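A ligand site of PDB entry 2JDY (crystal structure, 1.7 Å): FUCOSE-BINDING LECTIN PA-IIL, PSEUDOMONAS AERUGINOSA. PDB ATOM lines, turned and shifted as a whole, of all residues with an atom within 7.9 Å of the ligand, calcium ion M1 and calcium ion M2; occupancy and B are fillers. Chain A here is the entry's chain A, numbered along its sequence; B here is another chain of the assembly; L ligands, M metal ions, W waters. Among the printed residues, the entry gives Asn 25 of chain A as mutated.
The side-chain carboxylate (OD1) of Asp 97 sits close to an oxygen (O4) of the ligand (2.6 Å). An oxygen (O5) of the ligand lies within hydrogen-bond range of the backbone NH (N) of Ser 24, at 3.0 Å. An oxygen (O6) of the ligand lies within hydrogen-bond range of the side-chain hydroxyl of Ser 24 (2.7 Å). The side-chain amide nitrogen (ND2) of Asn 25 sits close to an oxygen (O6) of the ligand (3.3 Å).
O of Leu 114 of chain B lies close to ND2 of Asn 104. The side-chain amide nitrogen (ND2) of Asn 104 lies within hydrogen-bond range of the backbone carbonyl oxygen (O) of Pro 113 of chain B, at 2.7 Å. The side-chain carboxylate (OE1) of Glu 96 lies close to the backbone NH (N) of Tyr 103. The side-chain carboxylate (OE1) of Glu 96 sits close to the backbone NH (N) of Asn 101 (3.4 Å). The side-chain carboxylate (OD2) of Asp 97 sits at hydrogen-bond distance from the side-chain amide nitrogen (ND2) of Asn 25 (3.2 Å). OG of Ser 23 lies within hydrogen-bond range of OD2 of Asp 97 (2.7 Å). The side-chain amide nitrogen (NE2) of Gln 27 sits close to the side-chain hydroxyl (OG) of Ser 23, at 3.4 Å. O of Ser 45 is in hydrogen-bond range of N of Ser 23 (2.8 Å).
Merely in contact with the ligand: Ser 23. Ten residues have an atom within 4 Å of the ligand: Asn 22, Ser 23, Ser 24, Asn 25, Glu 96, Asp 97, Asp 100, Asp 102, Asp 105 and Gly 115 of chain B.
Five residues have an atom within 4 Å of calcium ion M1: Asn 22, Asp 102, Asn 104, Asp 105 and Gly 115 of chain B. The nearest printed residue that does not touch calcium ion M1 is Ser 23 (4.4 Å).
Within 4 Å of calcium ion M2: Glu 96, Asp 100, Asp 102 and Asp 105.
Calcium ion M1 is bound by the side-chain amide oxygen (OD1) of Asn 104 (2.3 Å), the backbone carbonyl oxygen (O) of Asn 22 (2.3 Å), the side-chain carboxylate (OD1) of Asp 105 (2.4 Å), the chain-end carboxylate (O) of Gly 115 of chain B (2.5 Å), the side-chain carboxylate (OD2) of Asp 102 (2.5 Å), an oxygen (O2) of the ligand (2.5 Å) and an oxygen (O3) of the ligand (2.5 Å). Slightly farther from calcium ion M1 lies the side-chain carboxylate (OD1) of Asp 102 (3.1 Å).
Calcium ion M2 is bound by OD1 of Asp 100 (2.3 Å). Calcium ion M2 is bound by OD1 of Asp 102. OE1 of Glu 96 is bound to calcium ion M2, 2.4 Å away. OE2 of Glu 96 is bound to calcium ion M2 (2.5 Å). Calcium ion M2 is bound by O3 of the ligand. OD2 of Asp 105 binds calcium ion M2 (2.5 Å). An oxygen (O4) of the ligand binds calcium ion M2 (2.6 Å). OD1 of Asp 105 is bound to calcium ion M2, 2.7 Å away. Calcium ion M2 has eight donor atoms within binding distance.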
ATOM      1  N   ALA A  21      -6.686 -15.635  -0.922  1.00  0.00           N
ATOM      2  CA  ALA A  21      -7.982 -14.953  -0.846  1.00  0.00           C
ATOM      3  C   ALA A  21      -8.007 -13.922   0.275  1.00  0.00           C
ATOM      4  O   ALA A  21      -7.417 -14.130   1.344  1.00  0.00           O
ATOM      5  CB  ALA A  21      -9.125 -15.972  -0.643  1.00  0.00           C
ATOM      6  N   ASN A  22      -8.637 -12.781  -0.006  1.00  0.00           N
ATOM      7  CA  ASN A  22      -8.805 -11.693   0.994  1.00  0.00           C
ATOM      8  C   ASN A  22     -10.166 -11.060   0.748  1.00  0.00           C
ATOM      9  O   ASN A  22     -10.255  -9.949   0.205  1.00  0.00           O
ATOM     10  CB  ASN A  22      -7.719 -10.621   0.859  1.00  0.00           C
ATOM     11  CG  ASN A  22      -6.360 -11.124   1.317  1.00  0.00           C
ATOM     12  OD1 ASN A  22      -6.087 -11.187   2.522  1.00  0.00           O
ATOM     13  ND2 ASN A  22      -5.502 -11.455   0.363  1.00  0.00           N
ATOM     14  N   SER A  23     -11.221 -11.789   1.081  1.00  0.00           N
ATOM     15  CA  SER A  23     -12.577 -11.350   0.767  1.00  0.00           C
ATOM     16  C   SER A  23     -13.619 -12.091   1.577  1.00  0.00           C
ATOM     17  O   SER A  23     -13.399 -13.248   1.944  1.00  0.00           O
ATOM     18  CB  SER A  23     -12.897 -11.515  -0.728  1.00  0.00           C
ATOM     19  OG  SER A  23     -14.194 -11.039  -1.036  1.00  0.00           O
ATOM     20  N   SER A  24     -14.749 -11.442   1.821  1.00  0.00           N
ATOM     21  CA  SER A  24     -15.906 -12.156   2.414  1.00  0.00           C
ATOM     22  C   SER A  24     -16.519 -13.139   1.381  1.00  0.00           C
ATOM     23  O   SER A  24     -17.077 -14.178   1.774  1.00  0.00           O
ATOM     24  CB  SER A  24     -16.957 -11.175   2.951  1.00  0.00           C
ATOM     25  OG  SER A  24     -17.669 -10.530   1.903  1.00  0.00           O
ATOM     26  N   ASN A  25     -16.363 -12.838   0.085  1.00  0.00           N
ATOM     27  CA  ASN A  25     -16.854 -13.718  -0.977  1.00  0.00           C
ATOM     28  C   ASN A  25     -15.935 -14.887  -1.242  1.00  0.00           C
ATOM     29  O   ASN A  25     -14.700 -14.761  -1.166  1.00  0.00           O
ATOM     30  CB  ASN A  25     -17.006 -12.948  -2.287  1.00  0.00           C
ATOM     31  CG  ASN A  25     -18.088 -11.877  -2.222  1.00  0.00           C
ATOM     32  OD1 ASN A  25     -19.150 -12.083  -1.607  1.00  0.00           O
ATOM     33  ND2 ASN A  25     -17.812 -10.718  -2.844  1.00  0.00           N
ATOM     34  N   THR A  26     -16.542 -16.030  -1.592  1.00  0.00           N
ATOM     35  CA  THR A  26     -15.755 -17.184  -2.009  1.00  0.00           C
ATOM     36  C   THR A  26     -15.216 -16.900  -3.411  1.00  0.00           C
ATOM     37  O   THR A  26     -15.990 -16.586  -4.319  1.00  0.00           O
ATOM     38  CB  THR A  26     -16.620 -18.438  -1.994  1.00  0.00           C
ATOM     39  OG1 THR A  26     -17.118 -18.605  -0.660  1.00  0.00           O
ATOM     40  CG2 THR A  26     -15.792 -19.659  -2.374  1.00  0.00           C
ATOM     41  N   GLN A  27     -13.912 -17.070  -3.576  1.00  0.00           N
ATOM     42  CA  GLN A  27     -13.237 -16.779  -4.849  1.00  0.00           C
ATOM     43  C   GLN A  27     -13.101 -18.035  -5.708  1.00  0.00           C
ATOM     44  O   GLN A  27     -12.866 -19.122  -5.171  1.00  0.00           O
ATOM     45  CB  GLN A  27     -11.820 -16.230  -4.578  1.00  0.00           C
ATOM     46  CG  GLN A  27     -11.810 -15.014  -3.660  1.00  0.00           C
ATOM     47  CD  GLN A  27     -12.468 -13.818  -4.285  1.00  0.00           C
ATOM     48  OE1 GLN A  27     -12.177 -13.488  -5.428  1.00  0.00           O
ATOM     49  NE2 GLN A  27     -13.368 -13.144  -3.530  1.00  0.00           N
ATOM     50  N   GLN A  44     -12.330 -19.267   0.639  1.00  0.00           N
ATOM     51  CA  GLN A  44     -12.703 -17.978   1.191  1.00  0.00           C
ATOM     52  C   GLN A  44     -11.855 -17.708   2.433  1.00  0.00           C
ATOM     53  O   GLN A  44     -11.687 -18.590   3.269  1.00  0.00           O
ATOM     54  CB  GLN A  44     -14.198 -18.030   1.581  1.00  0.00           C
ATOM     55  CG  GLN A  44     -14.768 -16.705   2.178  1.00  0.00           C
ATOM     56  CD  GLN A  44     -14.488 -16.504   3.669  1.00  0.00           C
ATOM     57  OE1 GLN A  44     -14.668 -17.409   4.500  1.00  0.00           O
ATOM     58  NE2 GLN A  44     -14.108 -15.271   4.029  1.00  0.00           N
ATOM     59  N   SER A  45     -11.317 -16.483   2.517  1.00  0.00           N
ATOM     60  CA  SER A  45     -10.502 -16.082   3.661  1.00  0.00           C
ATOM     61  C   SER A  45     -10.405 -14.585   3.621  1.00  0.00           C
ATOM     62  O   SER A  45     -10.348 -14.016   2.531  1.00  0.00           O
ATOM     63  CB  SER A  45      -9.091 -16.675   3.547  1.00  0.00           C
ATOM     64  OG  SER A  45      -8.271 -16.188   4.600  1.00  0.00           O
ATOM     65  N   THR A  46     -10.338 -13.953   4.784  1.00  0.00           N
ATOM     66  CA  THR A  46     -10.031 -12.539   4.864  1.00  0.00           C
ATOM     67  C   THR A  46      -8.609 -12.397   5.446  1.00  0.00           C
ATOM     68  O   THR A  46      -8.213 -11.319   5.887  1.00  0.00           O
ATOM     69  CB  THR A  46     -11.077 -11.772   5.731  1.00  0.00           C
ATOM     70  OG1 THR A  46     -11.256 -12.448   6.970  1.00  0.00           O
ATOM     71  CG2 THR A  46     -12.412 -11.658   4.991  1.00  0.00           C
ATOM     72  N   VAL A  70     -16.586 -14.425  -8.904  1.00  0.00           N
ATOM     73  CA  VAL A  70     -17.301 -14.558  -7.648  1.00  0.00           C
ATOM     74  C   VAL A  70     -18.789 -14.590  -8.012  1.00  0.00           C
ATOM     75  O   VAL A  70     -19.287 -13.678  -8.672  1.00  0.00           O
ATOM     76  CB  VAL A  70     -17.052 -13.347  -6.723  1.00  0.00           C
ATOM     77  CG1 VAL A  70     -18.012 -13.378  -5.525  1.00  0.00           C
ATOM     78  CG2 VAL A  70     -15.615 -13.368  -6.261  1.00  0.00           C
ATOM     79  N   SER A  95      -7.315  -8.793  -7.990  1.00  0.00           N
ATOM     80  CA  SER A  95      -8.671  -8.759  -8.509  1.00  0.00           C
ATOM     81  C   SER A  95      -9.604  -8.068  -7.512  1.00  0.00           C
ATOM     82  O   SER A  95      -9.395  -8.137  -6.297  1.00  0.00           O
ATOM     83  CB  SER A  95      -9.176 -10.158  -8.827  1.00  0.00           C
ATOM     84  OG  SER A  95      -9.218 -10.945  -7.668  1.00  0.00           O
ATOM     85  N   GLU A  96     -10.618  -7.394  -8.048  1.00  0.00           N
ATOM     86  CA  GLU A  96     -11.607  -6.692  -7.253  1.00  0.00           C
ATOM     87  C   GLU A  96     -13.012  -7.247  -7.527  1.00  0.00           C
ATOM     88  O   GLU A  96     -13.449  -7.305  -8.673  1.00  0.00           O
ATOM     89  CB  GLU A  96     -11.554  -5.193  -7.560  1.00  0.00           C
ATOM     90  CG  GLU A  96     -12.564  -4.344  -6.739  1.00  0.00           C
ATOM     91  CD  GLU A  96     -12.498  -4.613  -5.237  1.00  0.00           C
ATOM     92  OE1 GLU A  96     -11.390  -4.546  -4.649  1.00  0.00           O
ATOM     93  OE2 GLU A  96     -13.580  -4.894  -4.624  1.00  0.00           O
ATOM     94  N   ASP A  97     -13.701  -7.656  -6.455  1.00  0.00           N
ATOM     95  CA  ASP A  97     -15.008  -8.291  -6.591  1.00  0.00           C
ATOM     96  C   ASP A  97     -16.126  -7.383  -6.094  1.00  0.00           C
ATOM     97  O   ASP A  97     -17.295  -7.778  -6.120  1.00  0.00           O
ATOM     98  CB  ASP A  97     -15.020  -9.629  -5.839  1.00  0.00           C
ATOM     99  CG  ASP A  97     -14.922  -9.493  -4.308  1.00  0.00           C
ATOM    100  OD1 ASP A  97     -15.019  -8.344  -3.761  1.00  0.00           O
ATOM    101  OD2 ASP A  97     -14.739 -10.543  -3.654  1.00  0.00           O
ATOM    102  N   GLY A  98     -15.762  -6.189  -5.653  1.00  0.00           N
ATOM    103  CA  GLY A  98     -16.712  -5.310  -4.950  1.00  0.00           C
ATOM    104  C   GLY A  98     -16.475  -3.842  -5.222  1.00  0.00           C
ATOM    105  O   GLY A  98     -16.201  -3.434  -6.359  1.00  0.00           O
ATOM    106  N   THR A  99     -16.567  -3.065  -4.155  1.00  0.00           N
ATOM    107  CA  THR A  99     -16.623  -1.613  -4.242  1.00  0.00           C
ATOM    108  C   THR A  99     -15.519  -0.898  -3.474  1.00  0.00           C
ATOM    109  O   THR A  99     -15.389   0.334  -3.586  1.00  0.00           O
ATOM    110  CB  THR A  99     -17.991  -1.090  -3.753  1.00  0.00           C
ATOM    111  OG1 THR A  99     -18.226  -1.562  -2.415  1.00  0.00           O
ATOM    112  CG2 THR A  99     -19.122  -1.563  -4.727  1.00  0.00           C
ATOM    113  N   ASP A 100     -14.710  -1.625  -2.711  1.00  0.00           N
ATOM    114  CA  ASP A 100     -13.683  -0.983  -1.885  1.00  0.00           C
ATOM    115  C   ASP A 100     -12.332  -0.778  -2.598  1.00  0.00           C
ATOM    116  O   ASP A 100     -11.435  -0.110  -2.084  1.00  0.00           O
ATOM    117  CB  ASP A 100     -13.499  -1.711  -0.560  1.00  0.00           C
ATOM    118  CG  ASP A 100     -12.819  -3.064  -0.712  1.00  0.00           C
ATOM    119  OD1 ASP A 100     -12.923  -3.647  -1.821  1.00  0.00           O
ATOM    120  OD2 ASP A 100     -12.213  -3.534   0.275  1.00  0.00           O
ATOM    121  N   ASN A 101     -12.208  -1.392  -3.767  1.00  0.00           N
ATOM    122  CA  ASN A 101     -11.025  -1.216  -4.636  1.00  0.00           C
ATOM    123  C   ASN A 101      -9.703  -1.477  -3.925  1.00  0.00           C
ATOM    124  O   ASN A 101      -8.724  -0.753  -4.125  1.00  0.00           O
ATOM    125  CB  ASN A 101     -11.022   0.172  -5.283  1.00  0.00           C
ATOM    126  CG  ASN A 101     -12.136   0.310  -6.301  1.00  0.00           C
ATOM    127  OD1 ASN A 101     -12.759  -0.692  -6.735  1.00  0.00           O
ATOM    128  ND2 ASN A 101     -12.401   1.545  -6.714  1.00  0.00           N
ATOM    129  N   ASP A 102      -9.676  -2.518  -3.097  1.00  0.00           N
ATOM    130  CA  ASP A 102      -8.398  -3.003  -2.536  1.00  0.00           C
ATOM    131  C   ASP A 102      -7.661  -3.973  -3.493  1.00  0.00           C
ATOM    132  O   ASP A 102      -6.481  -4.205  -3.334  1.00  0.00           O
ATOM    133  CB  ASP A 102      -8.543  -3.526  -1.082  1.00  0.00           C
ATOM    134  CG  ASP A 102      -9.438  -4.764  -0.951  1.00  0.00           C
ATOM    135  OD1 ASP A 102     -10.042  -5.239  -1.954  1.00  0.00           O
ATOM    136  OD2 ASP A 102      -9.505  -5.336   0.176  1.00  0.00           O
ATOM    137  N   TYR A 103      -8.380  -4.534  -4.475  1.00  0.00           N
ATOM    138  CA  TYR A 103      -7.781  -5.393  -5.532  1.00  0.00           C
ATOM    139  C   TYR A 103      -7.008  -6.619  -5.011  1.00  0.00           C
ATOM    140  O   TYR A 103      -6.115  -7.135  -5.702  1.00  0.00           O
ATOM    141  CB  TYR A 103      -6.958  -4.567  -6.570  1.00  0.00           C
ATOM    142  CG  TYR A 103      -7.897  -3.918  -7.566  1.00  0.00           C
ATOM    143  CD1 TYR A 103      -8.201  -4.554  -8.781  1.00  0.00           C
ATOM    144  CD2 TYR A 103      -8.517  -2.694  -7.264  1.00  0.00           C
ATOM    145  CE1 TYR A 103      -9.097  -3.987  -9.666  1.00  0.00           C
ATOM    146  CE2 TYR A 103      -9.426  -2.121  -8.146  1.00  0.00           C
ATOM    147  CZ  TYR A 103      -9.703  -2.774  -9.350  1.00  0.00           C
ATOM    148  OH  TYR A 103     -10.616  -2.209 -10.228  1.00  0.00           O
ATOM    149  N   ASN A 104      -7.348  -7.079  -3.810  1.00  0.00           N
ATOM    150  CA  ASN A 104      -6.641  -8.217  -3.198  1.00  0.00           C
ATOM    151  C   ASN A 104      -7.591  -9.408  -2.982  1.00  0.00           C
ATOM    152  O   ASN A 104      -7.212 -10.404  -2.354  1.00  0.00           O
ATOM    153  CB  ASN A 104      -6.015  -7.772  -1.856  1.00  0.00           C
ATOM    154  CG  ASN A 104      -7.069  -7.540  -0.743  1.00  0.00           C
ATOM    155  OD1 ASN A 104      -8.276  -7.714  -0.980  1.00  0.00           O
ATOM    156  ND2 ASN A 104      -6.620  -7.155   0.471  1.00  0.00           N
ATOM    157  N   ASP A 105      -8.836  -9.297  -3.496  1.00  0.00           N
ATOM    158  CA  ASP A 105      -9.890 -10.292  -3.161  1.00  0.00           C
ATOM    159  C   ASP A 105      -9.472 -11.712  -3.555  1.00  0.00           C
ATOM    160  O   ASP A 105      -9.652 -12.648  -2.769  1.00  0.00           O
ATOM    161  CB  ASP A 105     -11.239  -9.898  -3.777  1.00  0.00           C
ATOM    162  CG  ASP A 105     -11.655  -8.513  -3.333  1.00  0.00           C
ATOM    163  OD1 ASP A 105     -11.479  -8.205  -2.104  1.00  0.00           O
ATOM    164  OD2 ASP A 105     -12.100  -7.725  -4.172  1.00  0.00           O
ATOM    165  N   ALA A 106      -8.881 -11.845  -4.731  1.00  0.00           N
ATOM    166  CA  ALA A 106      -8.037 -12.996  -5.044  1.00  0.00           C
ATOM    167  C   ALA A 106      -6.730 -12.467  -5.613  1.00  0.00           C
ATOM    168  O   ALA A 106      -6.718 -11.628  -6.549  1.00  0.00           O
ATOM    169  CB  ALA A 106      -8.702 -13.924  -6.074  1.00  0.00           C
ATOM    170  N   PRO B 113      -2.247  -4.700   0.756  1.00  0.00           N
ATOM    171  CA  PRO B 113      -2.871  -4.991   2.042  1.00  0.00           C
ATOM    172  C   PRO B 113      -3.680  -6.288   2.010  1.00  0.00           C
ATOM    173  O   PRO B 113      -3.971  -6.823   0.956  1.00  0.00           O
ATOM    174  CB  PRO B 113      -3.823  -3.814   2.246  1.00  0.00           C
ATOM    175  CG  PRO B 113      -4.175  -3.381   0.870  1.00  0.00           C
ATOM    176  CD  PRO B 113      -2.945  -3.625   0.034  1.00  0.00           C
ATOM    177  N   LEU B 114      -4.060  -6.761   3.199  1.00  0.00           N
ATOM    178  CA  LEU B 114      -4.870  -7.968   3.289  1.00  0.00           C
ATOM    179  C   LEU B 114      -6.306  -7.594   3.644  1.00  0.00           C
ATOM    180  O   LEU B 114      -6.613  -6.406   3.818  1.00  0.00           O
ATOM    181  CB  LEU B 114      -4.281  -8.896   4.351  1.00  0.00           C
ATOM    182  CG  LEU B 114      -2.809  -9.275   4.274  1.00  0.00           C
ATOM    183  CD1 LEU B 114      -2.461 -10.305   5.371  1.00  0.00           C
ATOM    184  CD2 LEU B 114      -2.462  -9.783   2.881  1.00  0.00           C
ATOM    185  N   GLY B 115      -7.170  -8.601   3.748  1.00  0.00           N
ATOM    186  CA  GLY B 115      -8.516  -8.405   4.274  1.00  0.00           C
ATOM    187  C   GLY B 115      -9.565  -8.180   3.221  1.00  0.00           C
ATOM    188  O   GLY B 115      -9.244  -7.741   2.088  1.00  0.00           O
ATOM    189  OXT GLY B 115     -10.756  -8.402   3.511  1.00  0.00           O
HETATM  190  C1  LIG L   1     -14.576  -7.777   2.296  1.00  0.00           C
HETATM  191  C2  LIG L   1     -13.311  -7.108   1.747  1.00  0.00           C
HETATM  192  C3  LIG L   1     -13.587  -6.405   0.417  1.00  0.00           C
HETATM  193  C4  LIG L   1     -14.276  -7.357  -0.558  1.00  0.00           C
HETATM  194  C5  LIG L   1     -15.569  -7.802   0.106  1.00  0.00           C
HETATM  195  C6  LIG L   1     -16.443  -8.669  -0.810  1.00  0.00           C
HETATM  196  C7  LIG L   1     -16.494  -7.237   3.604  1.00  0.00           C
HETATM  197  O1  LIG L   1     -15.474  -6.741   2.720  1.00  0.00           O
HETATM  198  O2  LIG L   1     -12.285  -8.109   1.532  1.00  0.00           O
HETATM  199  O3  LIG L   1     -12.335  -6.022  -0.188  1.00  0.00           O
HETATM  200  O4  LIG L   1     -14.492  -6.701  -1.840  1.00  0.00           O
HETATM  201  O5  LIG L   1     -15.229  -8.557   1.294  1.00  0.00           O
HETATM  202  O6  LIG L   1     -17.750  -8.762  -0.171  1.00  0.00           O
HETATM  203 CA    CA M   1     -10.403  -7.644  -0.070  1.00  0.00          CA
HETATM  204 CA    CA M   2     -12.232  -5.688  -2.675  1.00  0.00          CA
HETATM  205  O   HOH W   1     -14.356  -7.892   6.142  1.00  0.00           O
HETATM  206  O   HOH W   2     -15.320  -4.176   3.202  1.00  0.00           O
HETATM  207  O   HOH W   3     -16.150  -4.334  -1.535  1.00  0.00           O
HETATM  208  O   HOH W   4     -18.877  -5.977  -1.831  1.00  0.00           O
